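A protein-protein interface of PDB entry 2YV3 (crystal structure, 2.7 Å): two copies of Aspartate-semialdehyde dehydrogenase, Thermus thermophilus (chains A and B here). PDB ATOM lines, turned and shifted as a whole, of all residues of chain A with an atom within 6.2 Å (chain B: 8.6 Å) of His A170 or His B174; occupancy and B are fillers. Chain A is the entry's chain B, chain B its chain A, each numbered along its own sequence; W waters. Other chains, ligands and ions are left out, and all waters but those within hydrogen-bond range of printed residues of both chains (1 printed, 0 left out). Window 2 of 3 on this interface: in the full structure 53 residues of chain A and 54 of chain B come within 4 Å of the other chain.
A ring nitrogen (NE2) of His A174 lies close to a ring nitrogen (NE2) of His A170 (3.3 Å). The side-chain hydroxyl (OG1) of Thr A169 lies within hydrogen-bond range of the backbone carbonyl oxygen (O) of Leu A165, at 2.4 Å. A ring nitrogen (NE2) of His B170 lies close to a ring nitrogen (NE2) of His B174, at 3.4 Å.
His A170 touches two residues of chain B. His B174 touches just one residue of chain A: His A170. Thr A169 touches just these residues of chain B: Thr B169 and Phe B189. Of the printed residues of chain B, Leu A166 touches Leu B173. Printed residues of chain B within 4 Å of His A174: His B170 (3.6 Å). Printed residues of chain A within 4 Å of His B170: His A174. The nearest printed residue of chain B that does not touch Leu A165 is Leu B173 (5.9 Å).
Leu A166 touches Leu B173, and with the chains exchanged Leu A173 touches Leu B166. Thr A169 touches its own counterpart, Thr B169. His A170 touches Leu B173, but with the chains exchanged Leu A173 does not touch His B170 (4.4 Å). His A170 touches His B174, and with the chains exchanged His A174 touches His B170. Positions printed for both chains: 166, 167, 168, 169, 170, 171, 172, 173, 174, 175 and 176. Of the 8 pairs that touch across the chains among the printed residues, 5 have their exchanged pair printed and touching as well.
Of the 12 printed residues of chain A, 6 touch a printed residue of chain B. Hydrophobic or aromatic side chains of chain B within 4 Å of the printed part of chain A: His B170, Leu B173, His B174 and Phe B189. Among the printed residues, 8 pairs touch across the chains. Among the printed residues, no Asp or Glu carboxylate lies within 4 Å of a Lys or Arg side-chain nitrogen of the other chain.
Leu A165 touches Phe B189 (CD2 to CE1, 3.5 Å). CD2 of Leu A166 touches CD1 of Leu B173 (3.4 Å). CG2 of Thr A169 touches CG2 of Thr B169, at 3.5 Å. Phe B189 touches Thr A169 (CZ to OG1, 3.7 Å). His A170 touches Leu B173. His A170 touches His B174 (CE1 to CE1, 3.5 Å). O of Leu B166 touches CD1 of Leu A173, at 3.4 Å. His B170 touches His A174 (CE1 to CE1, 3.6 Å).
Water W1 lies within hydrogen-bond range of a ring nitrogen (NE2) of His B174 (2.7 Å), a ring nitrogen (NE2) of His A174 (2.8 Å), a ring nitrogen (NE2) of His A170 (2.8 Å) and a ring nitrogen (NE2) of His B170 (2.9 Å).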
ATOM      1  N   LEU A 165     -20.135  -5.861 -21.565  1.00  0.00           N
ATOM      2  CA  LEU A 165     -20.305  -6.353 -20.197  1.00  0.00           C
ATOM      3  C   LEU A 165     -18.973  -6.364 -19.438  1.00  0.00           C
ATOM      4  O   LEU A 165     -18.901  -5.927 -18.286  1.00  0.00           O
ATOM      5  CB  LEU A 165     -20.915  -7.764 -20.220  1.00  0.00           C
ATOM      6  CG  LEU A 165     -21.300  -8.447 -18.903  1.00  0.00           C
ATOM      7  CD1 LEU A 165     -22.412  -7.694 -18.215  1.00  0.00           C
ATOM      8  CD2 LEU A 165     -21.741  -9.872 -19.181  1.00  0.00           C
ATOM      9  N   LEU A 166     -17.921  -6.850 -20.089  1.00  0.00           N
ATOM     10  CA  LEU A 166     -16.606  -6.902 -19.468  1.00  0.00           C
ATOM     11  C   LEU A 166     -16.067  -5.529 -19.073  1.00  0.00           C
ATOM     12  O   LEU A 166     -15.786  -5.273 -17.899  1.00  0.00           O
ATOM     13  CB  LEU A 166     -15.606  -7.559 -20.414  1.00  0.00           C
ATOM     14  CG  LEU A 166     -15.759  -9.052 -20.678  1.00  0.00           C
ATOM     15  CD1 LEU A 166     -14.837  -9.441 -21.808  1.00  0.00           C
ATOM     16  CD2 LEU A 166     -15.452  -9.847 -19.413  1.00  0.00           C
ATOM     17  N   THR A 167     -15.924  -4.644 -20.054  1.00  0.00           N
ATOM     18  CA  THR A 167     -15.376  -3.315 -19.797  1.00  0.00           C
ATOM     19  C   THR A 167     -16.196  -2.449 -18.823  1.00  0.00           C
ATOM     20  O   THR A 167     -15.633  -1.623 -18.111  1.00  0.00           O
ATOM     21  CB  THR A 167     -15.137  -2.558 -21.145  1.00  0.00           C
ATOM     22  OG1 THR A 167     -14.854  -1.179 -20.888  1.00  0.00           O
ATOM     23  CG2 THR A 167     -16.340  -2.673 -22.048  1.00  0.00           C
ATOM     24  N   GLU A 168     -17.512  -2.654 -18.785  1.00  0.00           N
ATOM     25  CA  GLU A 168     -18.402  -1.895 -17.904  1.00  0.00           C
ATOM     26  C   GLU A 168     -18.302  -2.358 -16.456  1.00  0.00           C
ATOM     27  O   GLU A 168     -18.438  -1.569 -15.519  1.00  0.00           O
ATOM     28  CB  GLU A 168     -19.858  -2.012 -18.369  1.00  0.00           C
ATOM     29  CG  GLU A 168     -20.211  -1.158 -19.556  1.00  0.00           C
ATOM     30  CD  GLU A 168     -19.663   0.243 -19.432  1.00  0.00           C
ATOM     31  OE1 GLU A 168     -18.432   0.394 -19.343  1.00  0.00           O
ATOM     32  OE2 GLU A 168     -20.453   1.203 -19.422  1.00  0.00           O
ATOM     33  N   THR A 169     -18.112  -3.653 -16.268  1.00  0.00           N
ATOM     34  CA  THR A 169     -17.955  -4.181 -14.926  1.00  0.00           C
ATOM     35  C   THR A 169     -16.638  -3.565 -14.474  1.00  0.00           C
ATOM     36  O   THR A 169     -16.579  -2.859 -13.479  1.00  0.00           O
ATOM     37  CB  THR A 169     -17.816  -5.688 -14.966  1.00  0.00           C
ATOM     38  OG1 THR A 169     -18.756  -6.218 -15.903  1.00  0.00           O
ATOM     39  CG2 THR A 169     -18.094  -6.270 -13.611  1.00  0.00           C
ATOM     40  N   HIS A 170     -15.593  -3.826 -15.256  1.00  0.00           N
ATOM     41  CA  HIS A 170     -14.249  -3.309 -15.005  1.00  0.00           C
ATOM     42  C   HIS A 170     -14.352  -1.816 -14.652  1.00  0.00           C
ATOM     43  O   HIS A 170     -13.832  -1.345 -13.623  1.00  0.00           O
ATOM     44  CB  HIS A 170     -13.391  -3.512 -16.264  1.00  0.00           C
ATOM     45  CG  HIS A 170     -11.915  -3.445 -16.018  1.00  0.00           C
ATOM     46  ND1 HIS A 170     -11.023  -4.319 -16.602  1.00  0.00           N
ATOM     47  CD2 HIS A 170     -11.174  -2.609 -15.251  1.00  0.00           C
ATOM     48  CE1 HIS A 170      -9.797  -4.025 -16.204  1.00  0.00           C
ATOM     49  NE2 HIS A 170      -9.861  -2.991 -15.383  1.00  0.00           N
ATOM     50  N   ARG A 171     -15.039  -1.077 -15.510  1.00  0.00           N
ATOM     51  CA  ARG A 171     -15.219   0.337 -15.271  1.00  0.00           C
ATOM     52  C   ARG A 171     -15.912   0.524 -13.921  1.00  0.00           C
ATOM     53  O   ARG A 171     -15.461   1.298 -13.080  1.00  0.00           O
ATOM     54  CB  ARG A 171     -16.030   0.952 -16.410  1.00  0.00           C
ATOM     55  CG  ARG A 171     -15.237   1.136 -17.704  1.00  0.00           C
ATOM     56  CD  ARG A 171     -15.703   2.398 -18.386  1.00  0.00           C
ATOM     57  NE  ARG A 171     -15.936   3.428 -17.380  1.00  0.00           N
ATOM     58  CZ  ARG A 171     -16.679   4.515 -17.565  1.00  0.00           C
ATOM     59  NH1 ARG A 171     -17.276   4.738 -18.733  1.00  0.00           N
ATOM     60  NH2 ARG A 171     -16.841   5.381 -16.569  1.00  0.00           N
ATOM     61  N   PHE A 172     -16.991  -0.224 -13.713  1.00  0.00           N
ATOM     62  CA  PHE A 172     -17.744  -0.161 -12.470  1.00  0.00           C
ATOM     63  C   PHE A 172     -16.858  -0.503 -11.294  1.00  0.00           C
ATOM     64  O   PHE A 172     -16.789   0.254 -10.327  1.00  0.00           O
ATOM     65  CB  PHE A 172     -18.915  -1.142 -12.481  1.00  0.00           C
ATOM     66  CG  PHE A 172     -19.652  -1.213 -11.166  1.00  0.00           C
ATOM     67  CD1 PHE A 172     -20.803  -0.466 -10.953  1.00  0.00           C
ATOM     68  CD2 PHE A 172     -19.177  -2.011 -10.132  1.00  0.00           C
ATOM     69  CE1 PHE A 172     -21.469  -0.516  -9.738  1.00  0.00           C
ATOM     70  CE2 PHE A 172     -19.834  -2.067  -8.909  1.00  0.00           C
ATOM     71  CZ  PHE A 172     -20.988  -1.315  -8.713  1.00  0.00           C
ATOM     72  N   LEU A 173     -16.206  -1.661 -11.363  1.00  0.00           N
ATOM     73  CA  LEU A 173     -15.328  -2.086 -10.281  1.00  0.00           C
ATOM     74  C   LEU A 173     -14.412  -0.929  -9.892  1.00  0.00           C
ATOM     75  O   LEU A 173     -13.968  -0.849  -8.753  1.00  0.00           O
ATOM     76  CB  LEU A 173     -14.482  -3.314 -10.687  1.00  0.00           C
ATOM     77  CG  LEU A 173     -14.896  -4.753 -10.323  1.00  0.00           C
ATOM     78  CD1 LEU A 173     -15.601  -4.751  -8.965  1.00  0.00           C
ATOM     79  CD2 LEU A 173     -15.813  -5.342 -11.343  1.00  0.00           C
ATOM     80  N   HIS A 174     -14.151  -0.022 -10.832  1.00  0.00           N
ATOM     81  CA  HIS A 174     -13.280   1.110 -10.541  1.00  0.00           C
ATOM     82  C   HIS A 174     -13.948   2.386 -10.050  1.00  0.00           C
ATOM     83  O   HIS A 174     -13.323   3.447 -10.072  1.00  0.00           O
ATOM     84  CB  HIS A 174     -12.410   1.430 -11.749  1.00  0.00           C
ATOM     85  CG  HIS A 174     -11.333   0.422 -11.977  1.00  0.00           C
ATOM     86  ND1 HIS A 174     -10.414   0.089 -11.003  1.00  0.00           N
ATOM     87  CD2 HIS A 174     -11.039  -0.346 -13.052  1.00  0.00           C
ATOM     88  CE1 HIS A 174      -9.601  -0.843 -11.469  1.00  0.00           C
ATOM     89  NE2 HIS A 174      -9.958  -1.125 -12.709  1.00  0.00           N
ATOM     90  N   GLY A 175     -15.206   2.285  -9.616  1.00  0.00           N
ATOM     91  CA  GLY A 175     -15.911   3.440  -9.087  1.00  0.00           C
ATOM     92  C   GLY A 175     -16.523   4.421 -10.066  1.00  0.00           C
ATOM     93  O   GLY A 175     -16.875   5.541  -9.675  1.00  0.00           O
ATOM     94  N   GLU A 176     -16.654   4.026 -11.331  1.00  0.00           N
ATOM     95  CA  GLU A 176     -17.254   4.897 -12.335  1.00  0.00           C
ATOM     96  C   GLU A 176     -18.534   4.292 -12.899  1.00  0.00           C
ATOM     97  O   GLU A 176     -18.631   3.077 -13.064  1.00  0.00           O
ATOM     98  CB  GLU A 176     -16.259   5.181 -13.456  1.00  0.00           C
ATOM     99  CG  GLU A 176     -15.225   4.100 -13.634  1.00  0.00           C
ATOM    100  CD  GLU A 176     -14.273   4.390 -14.764  1.00  0.00           C
ATOM    101  OE1 GLU A 176     -13.314   3.606 -14.938  1.00  0.00           O
ATOM    102  OE2 GLU A 176     -14.476   5.394 -15.486  1.00  0.00           O
ATOM    103  N   LEU B 166     -16.497  -8.419  -5.522  1.00  0.00           N
ATOM    104  CA  LEU B 166     -15.806  -7.285  -6.095  1.00  0.00           C
ATOM    105  C   LEU B 166     -14.431  -7.715  -6.571  1.00  0.00           C
ATOM    106  O   LEU B 166     -14.092  -7.598  -7.752  1.00  0.00           O
ATOM    107  CB  LEU B 166     -15.653  -6.163  -5.055  1.00  0.00           C
ATOM    108  CG  LEU B 166     -16.907  -5.535  -4.431  1.00  0.00           C
ATOM    109  CD1 LEU B 166     -16.479  -4.620  -3.308  1.00  0.00           C
ATOM    110  CD2 LEU B 166     -17.733  -4.784  -5.488  1.00  0.00           C
ATOM    111  N   THR B 167     -13.645  -8.207  -5.623  1.00  0.00           N
ATOM    112  CA  THR B 167     -12.302  -8.664  -5.878  1.00  0.00           C
ATOM    113  C   THR B 167     -12.273  -9.780  -6.906  1.00  0.00           C
ATOM    114  O   THR B 167     -11.465  -9.755  -7.812  1.00  0.00           O
ATOM    115  CB  THR B 167     -11.637  -9.135  -4.562  1.00  0.00           C
ATOM    116  OG1 THR B 167     -10.430  -9.845  -4.849  1.00  0.00           O
ATOM    117  CG2 THR B 167     -12.564 -10.040  -3.794  1.00  0.00           C
ATOM    118  N   GLU B 168     -13.159 -10.754  -6.790  1.00  0.00           N
ATOM    119  CA  GLU B 168     -13.168 -11.854  -7.745  1.00  0.00           C
ATOM    120  C   GLU B 168     -13.498 -11.451  -9.174  1.00  0.00           C
ATOM    121  O   GLU B 168     -12.788 -11.826 -10.110  1.00  0.00           O
ATOM    122  CB  GLU B 168     -14.128 -12.952  -7.283  1.00  0.00           C
ATOM    123  CG  GLU B 168     -13.656 -13.682  -6.023  1.00  0.00           C
ATOM    124  CD  GLU B 168     -12.179 -14.094  -6.094  1.00  0.00           C
ATOM    125  OE1 GLU B 168     -11.321 -13.312  -5.615  1.00  0.00           O
ATOM    126  OE2 GLU B 168     -11.878 -15.187  -6.641  1.00  0.00           O
ATOM    127  N   THR B 169     -14.579 -10.697  -9.353  1.00  0.00           N
ATOM    128  CA  THR B 169     -14.961 -10.268 -10.689  1.00  0.00           C
ATOM    129  C   THR B 169     -13.787  -9.465 -11.239  1.00  0.00           C
ATOM    130  O   THR B 169     -13.597  -9.359 -12.450  1.00  0.00           O
ATOM    131  CB  THR B 169     -16.238  -9.384 -10.670  1.00  0.00           C
ATOM    132  OG1 THR B 169     -17.266 -10.025  -9.906  1.00  0.00           O
ATOM    133  CG2 THR B 169     -16.757  -9.170 -12.086  1.00  0.00           C
ATOM    134  N   HIS B 170     -12.985  -8.925 -10.328  1.00  0.00           N
ATOM    135  CA  HIS B 170     -11.832  -8.118 -10.705  1.00  0.00           C
ATOM    136  C   HIS B 170     -10.698  -8.950 -11.288  1.00  0.00           C
ATOM    137  O   HIS B 170     -10.136  -8.628 -12.342  1.00  0.00           O
ATOM    138  CB  HIS B 170     -11.317  -7.326  -9.500  1.00  0.00           C
ATOM    139  CG  HIS B 170     -10.582  -6.078  -9.883  1.00  0.00           C
ATOM    140  ND1 HIS B 170     -10.679  -4.904  -9.164  1.00  0.00           N
ATOM    141  CD2 HIS B 170      -9.761  -5.814 -10.928  1.00  0.00           C
ATOM    142  CE1 HIS B 170      -9.950  -3.971  -9.751  1.00  0.00           C
ATOM    143  NE2 HIS B 170      -9.384  -4.499 -10.825  1.00  0.00           N
ATOM    144  N   ARG B 171     -10.348 -10.016 -10.590  1.00  0.00           N
ATOM    145  CA  ARG B 171      -9.293 -10.885 -11.069  1.00  0.00           C
ATOM    146  C   ARG B 171      -9.778 -11.576 -12.347  1.00  0.00           C
ATOM    147  O   ARG B 171      -8.999 -11.789 -13.272  1.00  0.00           O
ATOM    148  CB  ARG B 171      -8.920 -11.875  -9.970  1.00  0.00           C
ATOM    149  CG  ARG B 171      -8.147 -11.238  -8.800  1.00  0.00           C
ATOM    150  CD  ARG B 171      -8.060 -12.231  -7.658  1.00  0.00           C
ATOM    151  NE  ARG B 171      -7.753 -13.568  -8.166  1.00  0.00           N
ATOM    152  CZ  ARG B 171      -8.125 -14.704  -7.580  1.00  0.00           C
ATOM    153  NH1 ARG B 171      -8.823 -14.669  -6.453  1.00  0.00           N
ATOM    154  NH2 ARG B 171      -7.805 -15.876  -8.125  1.00  0.00           N
ATOM    155  N   PHE B 172     -11.073 -11.884 -12.405  1.00  0.00           N
ATOM    156  CA  PHE B 172     -11.674 -12.499 -13.597  1.00  0.00           C
ATOM    157  C   PHE B 172     -11.273 -11.641 -14.817  1.00  0.00           C
ATOM    158  O   PHE B 172     -10.609 -12.119 -15.731  1.00  0.00           O
ATOM    159  CB  PHE B 172     -13.213 -12.534 -13.474  1.00  0.00           C
ATOM    160  CG  PHE B 172     -13.898 -13.221 -14.630  1.00  0.00           C
ATOM    161  CD1 PHE B 172     -13.918 -14.607 -14.723  1.00  0.00           C
ATOM    162  CD2 PHE B 172     -14.430 -12.479 -15.682  1.00  0.00           C
ATOM    163  CE1 PHE B 172     -14.444 -15.247 -15.853  1.00  0.00           C
ATOM    164  CE2 PHE B 172     -14.960 -13.111 -16.820  1.00  0.00           C
ATOM    165  CZ  PHE B 172     -14.964 -14.493 -16.907  1.00  0.00           C
ATOM    166  N   LEU B 173     -11.669 -10.369 -14.819  1.00  0.00           N
ATOM    167  CA  LEU B 173     -11.331  -9.461 -15.913  1.00  0.00           C
ATOM    168  C   LEU B 173      -9.852  -9.412 -16.254  1.00  0.00           C
ATOM    169  O   LEU B 173      -9.482  -8.970 -17.338  1.00  0.00           O
ATOM    170  CB  LEU B 173     -11.804  -8.045 -15.591  1.00  0.00           C
ATOM    171  CG  LEU B 173     -13.275  -7.785 -15.899  1.00  0.00           C
ATOM    172  CD1 LEU B 173     -13.496  -7.995 -17.397  1.00  0.00           C
ATOM    173  CD2 LEU B 173     -14.163  -8.718 -15.106  1.00  0.00           C
ATOM    174  N   HIS B 174      -9.010  -9.870 -15.335  1.00  0.00           N
ATOM    175  CA  HIS B 174      -7.567  -9.842 -15.549  1.00  0.00           C
ATOM    176  C   HIS B 174      -6.958 -11.187 -15.912  1.00  0.00           C
ATOM    177  O   HIS B 174      -5.742 -11.311 -16.032  1.00  0.00           O
ATOM    178  CB  HIS B 174      -6.867  -9.274 -14.314  1.00  0.00           C
ATOM    179  CG  HIS B 174      -7.093  -7.809 -14.117  1.00  0.00           C
ATOM    180  ND1 HIS B 174      -6.782  -6.874 -15.081  1.00  0.00           N
ATOM    181  CD2 HIS B 174      -7.588  -7.115 -13.066  1.00  0.00           C
ATOM    182  CE1 HIS B 174      -7.074  -5.667 -14.630  1.00  0.00           C
ATOM    183  NE2 HIS B 174      -7.565  -5.785 -13.410  1.00  0.00           N
ATOM    184  N   GLY B 175      -7.808 -12.195 -16.076  1.00  0.00           N
ATOM    185  CA  GLY B 175      -7.324 -13.506 -16.459  1.00  0.00           C
ATOM    186  C   GLY B 175      -7.321 -14.584 -15.402  1.00  0.00           C
ATOM    187  O   GLY B 175      -7.814 -15.684 -15.654  1.00  0.00           O
ATOM    188  N   GLU B 176      -6.776 -14.283 -14.224  1.00  0.00           N
ATOM    189  CA  GLU B 176      -6.692 -15.274 -13.159  1.00  0.00           C
ATOM    190  C   GLU B 176      -8.028 -15.886 -12.744  1.00  0.00           C
ATOM    191  O   GLU B 176      -9.005 -15.179 -12.510  1.00  0.00           O
ATOM    192  CB  GLU B 176      -5.938 -14.689 -11.949  1.00  0.00           C
ATOM    193  CG  GLU B 176      -6.321 -13.270 -11.530  1.00  0.00           C
ATOM    194  CD  GLU B 176      -5.297 -12.632 -10.567  1.00  0.00           C
ATOM    195  OE1 GLU B 176      -5.599 -11.568  -9.968  1.00  0.00           O
ATOM    196  OE2 GLU B 176      -4.179 -13.190 -10.419  1.00  0.00           O
ATOM    197  N   ALA B 177      -8.054 -17.217 -12.673  1.00  0.00           N
ATOM    198  CA  ALA B 177      -9.259 -17.972 -12.311  1.00  0.00           C
ATOM    199  C   ALA B 177      -9.781 -17.585 -10.943  1.00  0.00           C
ATOM    200  O   ALA B 177      -9.044 -17.616  -9.951  1.00  0.00           O
ATOM    201  CB  ALA B 177      -8.984 -19.481 -12.349  1.00  0.00           C
ATOM    202  N   PHE B 189     -19.687 -13.713 -12.946  1.00  0.00           N
ATOM    203  CA  PHE B 189     -20.251 -14.079 -14.246  1.00  0.00           C
ATOM    204  C   PHE B 189     -20.853 -15.470 -14.252  1.00  0.00           C
ATOM    205  O   PHE B 189     -20.553 -16.299 -15.103  1.00  0.00           O
ATOM    206  CB  PHE B 189     -19.173 -13.949 -15.314  1.00  0.00           C
ATOM    207  CG  PHE B 189     -18.832 -12.534 -15.627  1.00  0.00           C
ATOM    208  CD1 PHE B 189     -19.740 -11.732 -16.307  1.00  0.00           C
ATOM    209  CD2 PHE B 189     -17.641 -11.979 -15.195  1.00  0.00           C
ATOM    210  CE1 PHE B 189     -19.463 -10.395 -16.550  1.00  0.00           C
ATOM    211  CE2 PHE B 189     -17.354 -10.639 -15.434  1.00  0.00           C
ATOM    212  CZ  PHE B 189     -18.268  -9.846 -16.113  1.00  0.00           C
HETATM  213  O   HOH W   1      -8.211  -3.205 -13.141  1.00  0.00           O
